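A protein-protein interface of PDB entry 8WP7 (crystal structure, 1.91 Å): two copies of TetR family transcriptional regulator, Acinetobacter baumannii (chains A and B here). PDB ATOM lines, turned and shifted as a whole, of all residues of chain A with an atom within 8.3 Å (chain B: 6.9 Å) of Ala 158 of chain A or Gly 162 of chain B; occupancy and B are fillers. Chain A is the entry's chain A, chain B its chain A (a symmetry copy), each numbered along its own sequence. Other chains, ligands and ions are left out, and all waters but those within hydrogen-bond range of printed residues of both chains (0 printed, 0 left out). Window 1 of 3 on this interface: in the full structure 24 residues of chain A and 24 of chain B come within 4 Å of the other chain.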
ATOM      1  N   LEU A  87      -3.274  16.550   3.416  1.00  0.00           N
ATOM      2  CA  LEU A  87      -4.540  16.156   4.021  1.00  0.00           C
ATOM      3  C   LEU A  87      -5.406  15.285   3.116  1.00  0.00           C
ATOM      4  O   LEU A  87      -6.533  14.954   3.500  1.00  0.00           O
ATOM      5  CB  LEU A  87      -5.329  17.399   4.450  1.00  0.00           C
ATOM      6  CG  LEU A  87      -4.677  18.239   5.550  1.00  0.00           C
ATOM      7  CD1 LEU A  87      -5.406  19.555   5.708  1.00  0.00           C
ATOM      8  CD2 LEU A  87      -4.692  17.462   6.866  1.00  0.00           C
ATOM      9  N   MET A 123       0.988   7.919  11.979  1.00  0.00           N
ATOM     10  CA  MET A 123       0.144   9.045  12.371  1.00  0.00           C
ATOM     11  C   MET A 123       0.988  10.172  12.947  1.00  0.00           C
ATOM     12  O   MET A 123       0.747  11.350  12.659  1.00  0.00           O
ATOM     13  CB  MET A 123      -0.913   8.597  13.388  1.00  0.00           C
ATOM     14  CG  MET A 123      -2.041   7.778  12.775  1.00  0.00           C
ATOM     15  SD  MET A 123      -3.272   8.762  11.895  1.00  0.00           S
ATOM     16  CE  MET A 123      -3.414  10.170  12.988  1.00  0.00           C
ATOM     17  N   TRP A 126       2.718  11.861  10.039  1.00  0.00           N
ATOM     18  CA  TRP A 126       1.756  12.712   9.347  1.00  0.00           C
ATOM     19  C   TRP A 126       1.568  14.030  10.087  1.00  0.00           C
ATOM     20  O   TRP A 126       1.595  15.109   9.480  1.00  0.00           O
ATOM     21  CB  TRP A 126       0.425  11.965   9.227  1.00  0.00           C
ATOM     22  CG  TRP A 126      -0.628  12.613   8.366  1.00  0.00           C
ATOM     23  CD1 TRP A 126      -0.445  13.555   7.391  1.00  0.00           C
ATOM     24  CD2 TRP A 126      -2.038  12.352   8.417  1.00  0.00           C
ATOM     25  NE1 TRP A 126      -1.661  13.892   6.831  1.00  0.00           N
ATOM     26  CE2 TRP A 126      -2.652  13.168   7.446  1.00  0.00           C
ATOM     27  CE3 TRP A 126      -2.840  11.509   9.197  1.00  0.00           C
ATOM     28  CZ2 TRP A 126      -4.030  13.164   7.228  1.00  0.00           C
ATOM     29  CZ3 TRP A 126      -4.213  11.504   8.979  1.00  0.00           C
ATOM     30  CH2 TRP A 126      -4.792  12.328   8.002  1.00  0.00           C
ATOM     31  N   HIS A 127       1.375  13.958  11.406  1.00  0.00           N
ATOM     32  CA  HIS A 127       1.233  15.165  12.212  1.00  0.00           C
ATOM     33  C   HIS A 127       2.450  16.071  12.077  1.00  0.00           C
ATOM     34  O   HIS A 127       2.312  17.292  11.938  1.00  0.00           O
ATOM     35  CB  HIS A 127       1.001  14.790  13.677  1.00  0.00           C
ATOM     36  CG  HIS A 127       0.912  15.969  14.591  1.00  0.00           C
ATOM     37  ND1 HIS A 127       1.969  16.389  15.372  1.00  0.00           N
ATOM     38  CD2 HIS A 127      -0.104  16.828  14.840  1.00  0.00           C
ATOM     39  CE1 HIS A 127       1.604  17.450  16.068  1.00  0.00           C
ATOM     40  NE2 HIS A 127       0.352  17.737  15.763  1.00  0.00           N
ATOM     41  N   ILE A 130       2.508  17.925   8.772  1.00  0.00           N
ATOM     42  CA  ILE A 130       1.564  19.037   8.755  1.00  0.00           C
ATOM     43  C   ILE A 130       2.085  20.192   9.602  1.00  0.00           C
ATOM     44  O   ILE A 130       1.961  21.363   9.223  1.00  0.00           O
ATOM     45  CB  ILE A 130       0.182  18.551   9.224  1.00  0.00           C
ATOM     46  CG1 ILE A 130      -0.410  17.607   8.173  1.00  0.00           C
ATOM     47  CG2 ILE A 130      -0.759  19.737   9.457  1.00  0.00           C
ATOM     48  CD1 ILE A 130      -1.649  16.891   8.648  1.00  0.00           C
ATOM     49  N   ASP A 151      -1.321  22.421  17.764  1.00  0.00           N
ATOM     50  CA  ASP A 151      -2.763  22.347  17.971  1.00  0.00           C
ATOM     51  C   ASP A 151      -3.500  22.302  16.641  1.00  0.00           C
ATOM     52  O   ASP A 151      -4.425  21.503  16.455  1.00  0.00           O
ATOM     53  CB  ASP A 151      -3.243  23.550  18.787  1.00  0.00           C
ATOM     54  CG  ASP A 151      -3.000  23.391  20.275  1.00  0.00           C
ATOM     55  OD1 ASP A 151      -2.833  22.244  20.743  1.00  0.00           O
ATOM     56  OD2 ASP A 151      -2.999  24.425  20.981  1.00  0.00           O
ATOM     57  N   ILE A 152      -3.117  23.177  15.708  1.00  0.00           N
ATOM     58  CA  ILE A 152      -3.795  23.240  14.418  1.00  0.00           C
ATOM     59  C   ILE A 152      -3.617  21.935  13.659  1.00  0.00           C
ATOM     60  O   ILE A 152      -4.554  21.436  13.026  1.00  0.00           O
ATOM     61  CB  ILE A 152      -3.278  24.438  13.598  1.00  0.00           C
ATOM     62  CG1 ILE A 152      -3.544  25.750  14.343  1.00  0.00           C
ATOM     63  CG2 ILE A 152      -3.924  24.452  12.214  1.00  0.00           C
ATOM     64  CD1 ILE A 152      -2.828  26.957  13.737  1.00  0.00           C
ATOM     65  N   ALA A 153      -2.413  21.363  13.708  1.00  0.00           N
ATOM     66  CA  ALA A 153      -2.155  20.124  12.985  1.00  0.00           C
ATOM     67  C   ALA A 153      -3.042  18.990  13.486  1.00  0.00           C
ATOM     68  O   ALA A 153      -3.598  18.230  12.685  1.00  0.00           O
ATOM     69  CB  ALA A 153      -0.683  19.745  13.106  1.00  0.00           C
ATOM     70  N   TRP A 154      -3.178  18.844  14.808  1.00  0.00           N
ATOM     71  CA  TRP A 154      -4.056  17.793  15.316  1.00  0.00           C
ATOM     72  C   TRP A 154      -5.507  18.062  14.934  1.00  0.00           C
ATOM     73  O   TRP A 154      -6.244  17.135  14.575  1.00  0.00           O
ATOM     74  CB  TRP A 154      -3.912  17.646  16.835  1.00  0.00           C
ATOM     75  CG  TRP A 154      -2.678  16.879  17.276  1.00  0.00           C
ATOM     76  CD1 TRP A 154      -1.723  17.302  18.154  1.00  0.00           C
ATOM     77  CD2 TRP A 154      -2.275  15.569  16.847  1.00  0.00           C
ATOM     78  NE1 TRP A 154      -0.754  16.335  18.302  1.00  0.00           N
ATOM     79  CE2 TRP A 154      -1.069  15.262  17.511  1.00  0.00           C
ATOM     80  CE3 TRP A 154      -2.817  14.625  15.967  1.00  0.00           C
ATOM     81  CZ2 TRP A 154      -0.395  14.058  17.323  1.00  0.00           C
ATOM     82  CZ3 TRP A 154      -2.144  13.425  15.782  1.00  0.00           C
ATOM     83  CH2 TRP A 154      -0.945  13.155  16.456  1.00  0.00           C
ATOM     84  N   ARG A 155      -5.929  19.327  14.978  1.00  0.00           N
ATOM     85  CA  ARG A 155      -7.303  19.653  14.603  1.00  0.00           C
ATOM     86  C   ARG A 155      -7.567  19.358  13.130  1.00  0.00           C
ATOM     87  O   ARG A 155      -8.650  18.881  12.770  1.00  0.00           O
ATOM     88  CB  ARG A 155      -7.588  21.119  14.925  1.00  0.00           C
ATOM     89  CG  ARG A 155      -7.657  21.406  16.423  1.00  0.00           C
ATOM     90  CD  ARG A 155      -8.576  22.575  16.719  1.00  0.00           C
ATOM     91  NE  ARG A 155      -7.978  23.854  16.354  1.00  0.00           N
ATOM     92  CZ  ARG A 155      -7.310  24.641  17.188  1.00  0.00           C
ATOM     93  NH1 ARG A 155      -7.100  24.297  18.449  1.00  0.00           N
ATOM     94  NH2 ARG A 155      -6.848  25.810  16.747  1.00  0.00           N
ATOM     95  N   LEU A 156      -6.597  19.649  12.259  1.00  0.00           N
ATOM     96  CA  LEU A 156      -6.752  19.343  10.839  1.00  0.00           C
ATOM     97  C   LEU A 156      -6.841  17.838  10.612  1.00  0.00           C
ATOM     98  O   LEU A 156      -7.704  17.359   9.867  1.00  0.00           O
ATOM     99  CB  LEU A 156      -5.586  19.941  10.049  1.00  0.00           C
ATOM    100  CG  LEU A 156      -5.565  21.468   9.939  1.00  0.00           C
ATOM    101  CD1 LEU A 156      -4.365  21.956   9.116  1.00  0.00           C
ATOM    102  CD2 LEU A 156      -6.873  21.976   9.341  1.00  0.00           C
ATOM    103  N   ILE A 157      -5.956  17.073  11.256  1.00  0.00           N
ATOM    104  CA  ILE A 157      -6.008  15.619  11.129  1.00  0.00           C
ATOM    105  C   ILE A 157      -7.334  15.089  11.649  1.00  0.00           C
ATOM    106  O   ILE A 157      -7.973  14.239  11.015  1.00  0.00           O
ATOM    107  CB  ILE A 157      -4.817  14.973  11.858  1.00  0.00           C
ATOM    108  CG1 ILE A 157      -3.558  15.076  11.004  1.00  0.00           C
ATOM    109  CG2 ILE A 157      -5.121  13.516  12.193  1.00  0.00           C
ATOM    110  CD1 ILE A 157      -2.288  14.737  11.761  1.00  0.00           C
ATOM    111  N   ALA A 158      -7.775  15.587  12.804  1.00  0.00           N
ATOM    112  CA  ALA A 158      -9.047  15.139  13.356  1.00  0.00           C
ATOM    113  C   ALA A 158     -10.184  15.417  12.385  1.00  0.00           C
ATOM    114  O   ALA A 158     -11.067  14.573  12.187  1.00  0.00           O
ATOM    115  CB  ALA A 158      -9.305  15.824  14.701  1.00  0.00           C
ATOM    116  N   PHE A 159     -10.163  16.585  11.745  1.00  0.00           N
ATOM    117  CA  PHE A 159     -11.240  16.931  10.824  1.00  0.00           C
ATOM    118  C   PHE A 159     -11.315  15.959   9.656  1.00  0.00           C
ATOM    119  O   PHE A 159     -12.386  15.415   9.361  1.00  0.00           O
ATOM    120  CB  PHE A 159     -11.079  18.353  10.300  1.00  0.00           C
ATOM    121  CG  PHE A 159     -12.169  18.739   9.355  1.00  0.00           C
ATOM    122  CD1 PHE A 159     -13.434  19.049   9.834  1.00  0.00           C
ATOM    123  CD2 PHE A 159     -11.950  18.741   7.989  1.00  0.00           C
ATOM    124  CE1 PHE A 159     -14.458  19.383   8.958  1.00  0.00           C
ATOM    125  CE2 PHE A 159     -12.967  19.075   7.110  1.00  0.00           C
ATOM    126  CZ  PHE A 159     -14.221  19.397   7.596  1.00  0.00           C
ATOM    127  N   VAL A 160     -10.199  15.756   8.949  1.00  0.00           N
ATOM    128  CA  VAL A 160     -10.261  14.939   7.740  1.00  0.00           C
ATOM    129  C   VAL A 160     -10.534  13.481   8.087  1.00  0.00           C
ATOM    130  O   VAL A 160     -11.261  12.792   7.366  1.00  0.00           O
ATOM    131  CB  VAL A 160      -8.992  15.109   6.877  1.00  0.00           C
ATOM    132  CG1 VAL A 160      -8.795  16.575   6.498  1.00  0.00           C
ATOM    133  CG2 VAL A 160      -7.756  14.597   7.605  1.00  0.00           C
ATOM    134  N   CYS A 161      -9.987  12.989   9.201  1.00  0.00           N
ATOM    135  CA  CYS A 161     -10.315  11.628   9.620  1.00  0.00           C
ATOM    136  C   CYS A 161     -11.784  11.510  10.002  1.00  0.00           C
ATOM    137  O   CYS A 161     -12.445  10.527   9.651  1.00  0.00           O
ATOM    138  CB  CYS A 161      -9.428  11.195  10.785  1.00  0.00           C
ATOM    139  SG  CYS A 161      -7.681  11.007  10.372  1.00  0.00           S
ATOM    140  N   GLY A 162     -12.310  12.503  10.720  1.00  0.00           N
ATOM    141  CA  GLY A 162     -13.716  12.474  11.085  1.00  0.00           C
ATOM    142  C   GLY A 162     -14.637  12.595   9.888  1.00  0.00           C
ATOM    143  O   GLY A 162     -15.698  11.967   9.846  1.00  0.00           O
ATOM    144  N   LEU A 163     -14.251  13.401   8.899  1.00  0.00           N
ATOM    145  CA  LEU A 163     -15.100  13.554   7.720  1.00  0.00           C
ATOM    146  C   LEU A 163     -15.151  12.262   6.912  1.00  0.00           C
ATOM    147  O   LEU A 163     -16.228  11.837   6.473  1.00  0.00           O
ATOM    148  CB  LEU A 163     -14.601  14.724   6.868  1.00  0.00           C
ATOM    149  CG  LEU A 163     -15.541  15.241   5.780  1.00  0.00           C
ATOM    150  CD1 LEU A 163     -16.969  15.353   6.304  1.00  0.00           C
ATOM    151  CD2 LEU A 163     -15.043  16.574   5.230  1.00  0.00           C
ATOM    152  N   GLU A 164     -14.000  11.615   6.720  1.00  0.00           N
ATOM    153  CA  GLU A 164     -13.980  10.310   6.063  1.00  0.00           C
ATOM    154  C   GLU A 164     -14.798   9.284   6.836  1.00  0.00           C
ATOM    155  O   GLU A 164     -15.465   8.430   6.237  1.00  0.00           O
ATOM    156  CB  GLU A 164     -12.541   9.819   5.918  1.00  0.00           C
ATOM    157  CG  GLU A 164     -11.622  10.768   5.187  1.00  0.00           C
ATOM    158  CD  GLU A 164     -10.163  10.438   5.438  1.00  0.00           C
ATOM    159  OE1 GLU A 164      -9.309  11.338   5.282  1.00  0.00           O
ATOM    160  OE2 GLU A 164      -9.878   9.277   5.802  1.00  0.00           O
ATOM    161  N   GLY A 165     -14.737   9.329   8.167  1.00  0.00           N
ATOM    162  CA  GLY A 165     -15.532   8.404   8.962  1.00  0.00           C
ATOM    163  C   GLY A 165     -17.023   8.591   8.754  1.00  0.00           C
ATOM    164  O   GLY A 165     -17.784   7.620   8.722  1.00  0.00           O
ATOM    165  N   ILE A 166     -17.461   9.841   8.603  1.00  0.00           N
ATOM    166  CA  ILE A 166     -18.876  10.118   8.394  1.00  0.00           C
ATOM    167  C   ILE A 166     -19.312   9.636   7.015  1.00  0.00           C
ATOM    168  O   ILE A 166     -20.426   9.123   6.841  1.00  0.00           O
ATOM    169  CB  ILE A 166     -19.150  11.621   8.586  1.00  0.00           C
ATOM    170  CG1 ILE A 166     -18.975  12.013  10.053  1.00  0.00           C
ATOM    171  CG2 ILE A 166     -20.559  11.953   8.194  1.00  0.00           C
ATOM    172  CD1 ILE A 166     -19.848  11.229  10.995  1.00  0.00           C
ATOM    173  N   ILE A 186     -11.925  24.723   6.391  1.00  0.00           N
ATOM    174  CA  ILE A 186     -11.274  24.607   7.693  1.00  0.00           C
ATOM    175  C   ILE A 186      -9.849  25.151   7.639  1.00  0.00           C
ATOM    176  O   ILE A 186      -9.410  25.855   8.554  1.00  0.00           O
ATOM    177  CB  ILE A 186     -11.315  23.150   8.190  1.00  0.00           C
ATOM    178  CG1 ILE A 186     -12.766  22.691   8.356  1.00  0.00           C
ATOM    179  CG2 ILE A 186     -10.567  23.007   9.507  1.00  0.00           C
ATOM    180  CD1 ILE A 186     -13.521  23.457   9.424  1.00  0.00           C
ATOM    181  N   LEU B 156     -18.828  20.380  12.125  1.00  0.00           N
ATOM    182  CA  LEU B 156     -18.700  20.241  13.573  1.00  0.00           C
ATOM    183  C   LEU B 156     -18.790  18.778  13.992  1.00  0.00           C
ATOM    184  O   LEU B 156     -17.985  18.298  14.799  1.00  0.00           O
ATOM    185  CB  LEU B 156     -19.780  21.071  14.272  1.00  0.00           C
ATOM    186  CG  LEU B 156     -19.617  22.591  14.186  1.00  0.00           C
ATOM    187  CD1 LEU B 156     -20.743  23.320  14.931  1.00  0.00           C
ATOM    188  CD2 LEU B 156     -18.252  23.011  14.724  1.00  0.00           C
ATOM    189  N   ILE B 157     -19.765  18.049  13.444  1.00  0.00           N
ATOM    190  CA  ILE B 157     -19.887  16.627  13.757  1.00  0.00           C
ATOM    191  C   ILE B 157     -18.639  15.880  13.319  1.00  0.00           C
ATOM    192  O   ILE B 157     -18.102  15.047  14.061  1.00  0.00           O
ATOM    193  CB  ILE B 157     -21.153  16.041  13.106  1.00  0.00           C
ATOM    194  CG1 ILE B 157     -22.384  16.403  13.931  1.00  0.00           C
ATOM    195  CG2 ILE B 157     -21.029  14.527  12.963  1.00  0.00           C
ATOM    196  CD1 ILE B 157     -23.691  16.125  13.213  1.00  0.00           C
ATOM    197  N   ALA B 158     -18.151  16.170  12.112  1.00  0.00           N
ATOM    198  CA  ALA B 158     -16.946  15.506  11.632  1.00  0.00           C
ATOM    199  C   ALA B 158     -15.775  15.767  12.568  1.00  0.00           C
ATOM    200  O   ALA B 158     -14.999  14.855  12.879  1.00  0.00           O
ATOM    201  CB  ALA B 158     -16.618  15.978  10.213  1.00  0.00           C
ATOM    202  N   PHE B 159     -15.652  17.001  13.054  1.00  0.00           N
ATOM    203  CA  PHE B 159     -14.534  17.330  13.931  1.00  0.00           C
ATOM    204  C   PHE B 159     -14.567  16.513  15.214  1.00  0.00           C
ATOM    205  O   PHE B 159     -13.567  15.887  15.584  1.00  0.00           O
ATOM    206  CB  PHE B 159     -14.519  18.816  14.268  1.00  0.00           C
ATOM    207  CG  PHE B 159     -13.384  19.187  15.165  1.00  0.00           C
ATOM    208  CD1 PHE B 159     -12.094  19.278  14.660  1.00  0.00           C
ATOM    209  CD2 PHE B 159     -13.590  19.389  16.517  1.00  0.00           C
ATOM    210  CE1 PHE B 159     -11.030  19.596  15.493  1.00  0.00           C
ATOM    211  CE2 PHE B 159     -12.534  19.708  17.354  1.00  0.00           C
ATOM    212  CZ  PHE B 159     -11.253  19.813  16.840  1.00  0.00           C
ATOM    213  N   VAL B 160     -15.693  16.538  15.933  1.00  0.00           N
ATOM    214  CA  VAL B 160     -15.720  15.881  17.236  1.00  0.00           C
ATOM    215  C   VAL B 160     -15.628  14.368  17.081  1.00  0.00           C
ATOM    216  O   VAL B 160     -14.983  13.695  17.890  1.00  0.00           O
ATOM    217  CB  VAL B 160     -16.953  16.311  18.061  1.00  0.00           C
ATOM    218  CG1 VAL B 160     -16.970  17.825  18.249  1.00  0.00           C
ATOM    219  CG2 VAL B 160     -18.248  15.862  17.396  1.00  0.00           C
ATOM    220  N   CYS B 161     -16.238  13.807  16.035  1.00  0.00           N
ATOM    221  CA  CYS B 161     -16.079  12.374  15.796  1.00  0.00           C
ATOM    222  C   CYS B 161     -14.638  12.033  15.443  1.00  0.00           C
ATOM    223  O   CYS B 161     -14.096  11.031  15.922  1.00  0.00           O
ATOM    224  CB  CYS B 161     -17.020  11.905  14.689  1.00  0.00           C
ATOM    225  SG  CYS B 161     -18.775  11.983  15.109  1.00  0.00           S
ATOM    226  N   GLY B 162     -14.002  12.856  14.609  1.00  0.00           N
ATOM    227  CA  GLY B 162     -12.613  12.612  14.261  1.00  0.00           C
ATOM    228  C   GLY B 162     -11.675  12.773  15.440  1.00  0.00           C
ATOM    229  O   GLY B 162     -10.697  12.033  15.570  1.00  0.00           O
ATOM    230  N   LEU B 163     -11.954  13.739  16.315  1.00  0.00           N
ATOM    231  CA  LEU B 163     -11.083  13.939  17.471  1.00  0.00           C
ATOM    232  C   LEU B 163     -11.181  12.764  18.438  1.00  0.00           C
ATOM    233  O   LEU B 163     -10.159  12.272  18.936  1.00  0.00           O
ATOM    234  CB  LEU B 163     -11.431  15.259  18.163  1.00  0.00           C
ATOM    235  CG  LEU B 163     -10.427  15.794  19.184  1.00  0.00           C
ATOM    236  CD1 LEU B 163      -9.001  15.666  18.660  1.00  0.00           C
ATOM    237  CD2 LEU B 163     -10.759  17.237  19.555  1.00  0.00           C
ATOM    238  N   GLU B 164     -12.400  12.290  18.702  1.00  0.00           N
ATOM    239  CA  GLU B 164     -12.572  11.091  19.520  1.00  0.00           C
ATOM    240  C   GLU B 164     -11.889   9.884  18.891  1.00  0.00           C
ATOM    241  O   GLU B 164     -11.324   9.040  19.599  1.00  0.00           O
ATOM    242  CB  GLU B 164     -14.057  10.799  19.716  1.00  0.00           C
ATOM    243  CG  GLU B 164     -14.850  11.937  20.313  1.00  0.00           C
ATOM    244  CD  GLU B 164     -16.340  11.755  20.094  1.00  0.00           C
ATOM    245  OE1 GLU B 164     -17.080  12.764  20.128  1.00  0.00           O
ATOM    246  OE2 GLU B 164     -16.765  10.600  19.879  1.00  0.00           O
ATOM    247  N   GLY B 165     -11.954   9.765  17.565  1.00  0.00           N
ATOM    248  CA  GLY B 165     -11.281   8.658  16.901  1.00  0.00           C
ATOM    249  C   GLY B 165      -9.778   8.690  17.095  1.00  0.00           C
ATOM    250  O   GLY B 165      -9.138   7.647  17.256  1.00  0.00           O
ATOM    251  N   ILE B 166      -9.192   9.887  17.088  1.00  0.00           N
ATOM    252  CA  ILE B 166      -7.752  10.017  17.271  1.00  0.00           C
ATOM    253  C   ILE B 166      -7.366   9.666  18.704  1.00  0.00           C
ATOM    254  O   ILE B 166      -6.321   9.050  18.950  1.00  0.00           O
ATOM    255  CB  ILE B 166      -7.301  11.439  16.890  1.00  0.00           C
ATOM    256  CG1 ILE B 166      -7.439  11.659  15.384  1.00  0.00           C
ATOM    257  CG2 ILE B 166      -5.860  11.647  17.247  1.00  0.00           C
ATOM    258  CD1 ILE B 166      -6.674  10.662  14.557  1.00  0.00           C
ATOM    259  N   TYR B 167      -8.203  10.060  19.672  1.00  0.00           N
ATOM    260  CA  TYR B 167      -7.954   9.698  21.066  1.00  0.00           C
ATOM    261  C   TYR B 167      -7.949   8.191  21.265  1.00  0.00           C
ATOM    262  O   TYR B 167      -7.192   7.679  22.099  1.00  0.00           O
ATOM    263  CB  TYR B 167      -9.015  10.315  21.977  1.00  0.00           C
ATOM    264  CG  TYR B 167      -8.953  11.814  22.071  1.00  0.00           C
ATOM    265  CD1 TYR B 167      -7.761  12.495  21.878  1.00  0.00           C
ATOM    266  CD2 TYR B 167     -10.094  12.554  22.348  1.00  0.00           C
ATOM    267  CE1 TYR B 167      -7.707  13.865  21.965  1.00  0.00           C
ATOM    268  CE2 TYR B 167     -10.049  13.921  22.435  1.00  0.00           C
ATOM    269  CZ  TYR B 167      -8.856  14.573  22.245  1.00  0.00           C
ATOM    270  OH  TYR B 167      -8.812  15.945  22.328  1.00  0.00           O
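Among the printed residues, pairs that only touch across the chains: Gly 162 of chain A with Ala 158 of chain B, Ala 158 of chain A with Gly 162 of chain B, Gly 162 of chain A with Gly 162 of chain B, Met 123 of chain A with Ile 166 of chain B, Arg 155 of chain A with Phe 159 of chain B, Ala 158 of chain A with Leu 163 of chain B and Leu 163 of chain A with Ala 158 of chain B.
Of the printed residues of chain B, Met 123 of chain A touches Ile 166.
Leu 156 of chain A touches none of the printed residues of chain B.
Of the printed residues of chain B, Gly 162 of chain A touches Ala 158 (3.2 Å) and Gly 162 (3.4 Å).
Of the printed residues of chain B, Leu 163 of chain A touches Ala 158 (3.7 Å).
Val 160 of chain B touches none of the printed residues of chain A.
Of the 22 printed residues of chain A, 5 touch a printed residue of chain B.
Hydrophobic or aromatic side chains of chain A that line the printed part of chain B: Met 123, Ala 158 and Leu 163.
Among the printed residues, 7 pairs touch across the chains.
Among the printed residues, no Asp or Glu carboxylate lies within 4 Å of a Lys or Arg side-chain nitrogen of the other chain.
Ala 158 of chain A touches Gly 162 of chain B, and with the chains exchanged Gly 162 of chain A touches Ala 158 of chain B.
Ala 158 of chain A touches Leu 163 of chain B, and with the chains exchanged Leu 163 of chain A touches Ala 158 of chain B.
Gly 162 of chain A touches its own counterpart, Gly 162 of chain B.
Positions printed for both chains: 156, 157, 158, 159, 160, 161, 162, 163, 164, 165 and 166.
Of the 7 pairs that touch across the chains among the printed residues, 5 have their exchanged pair printed and touching as well.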
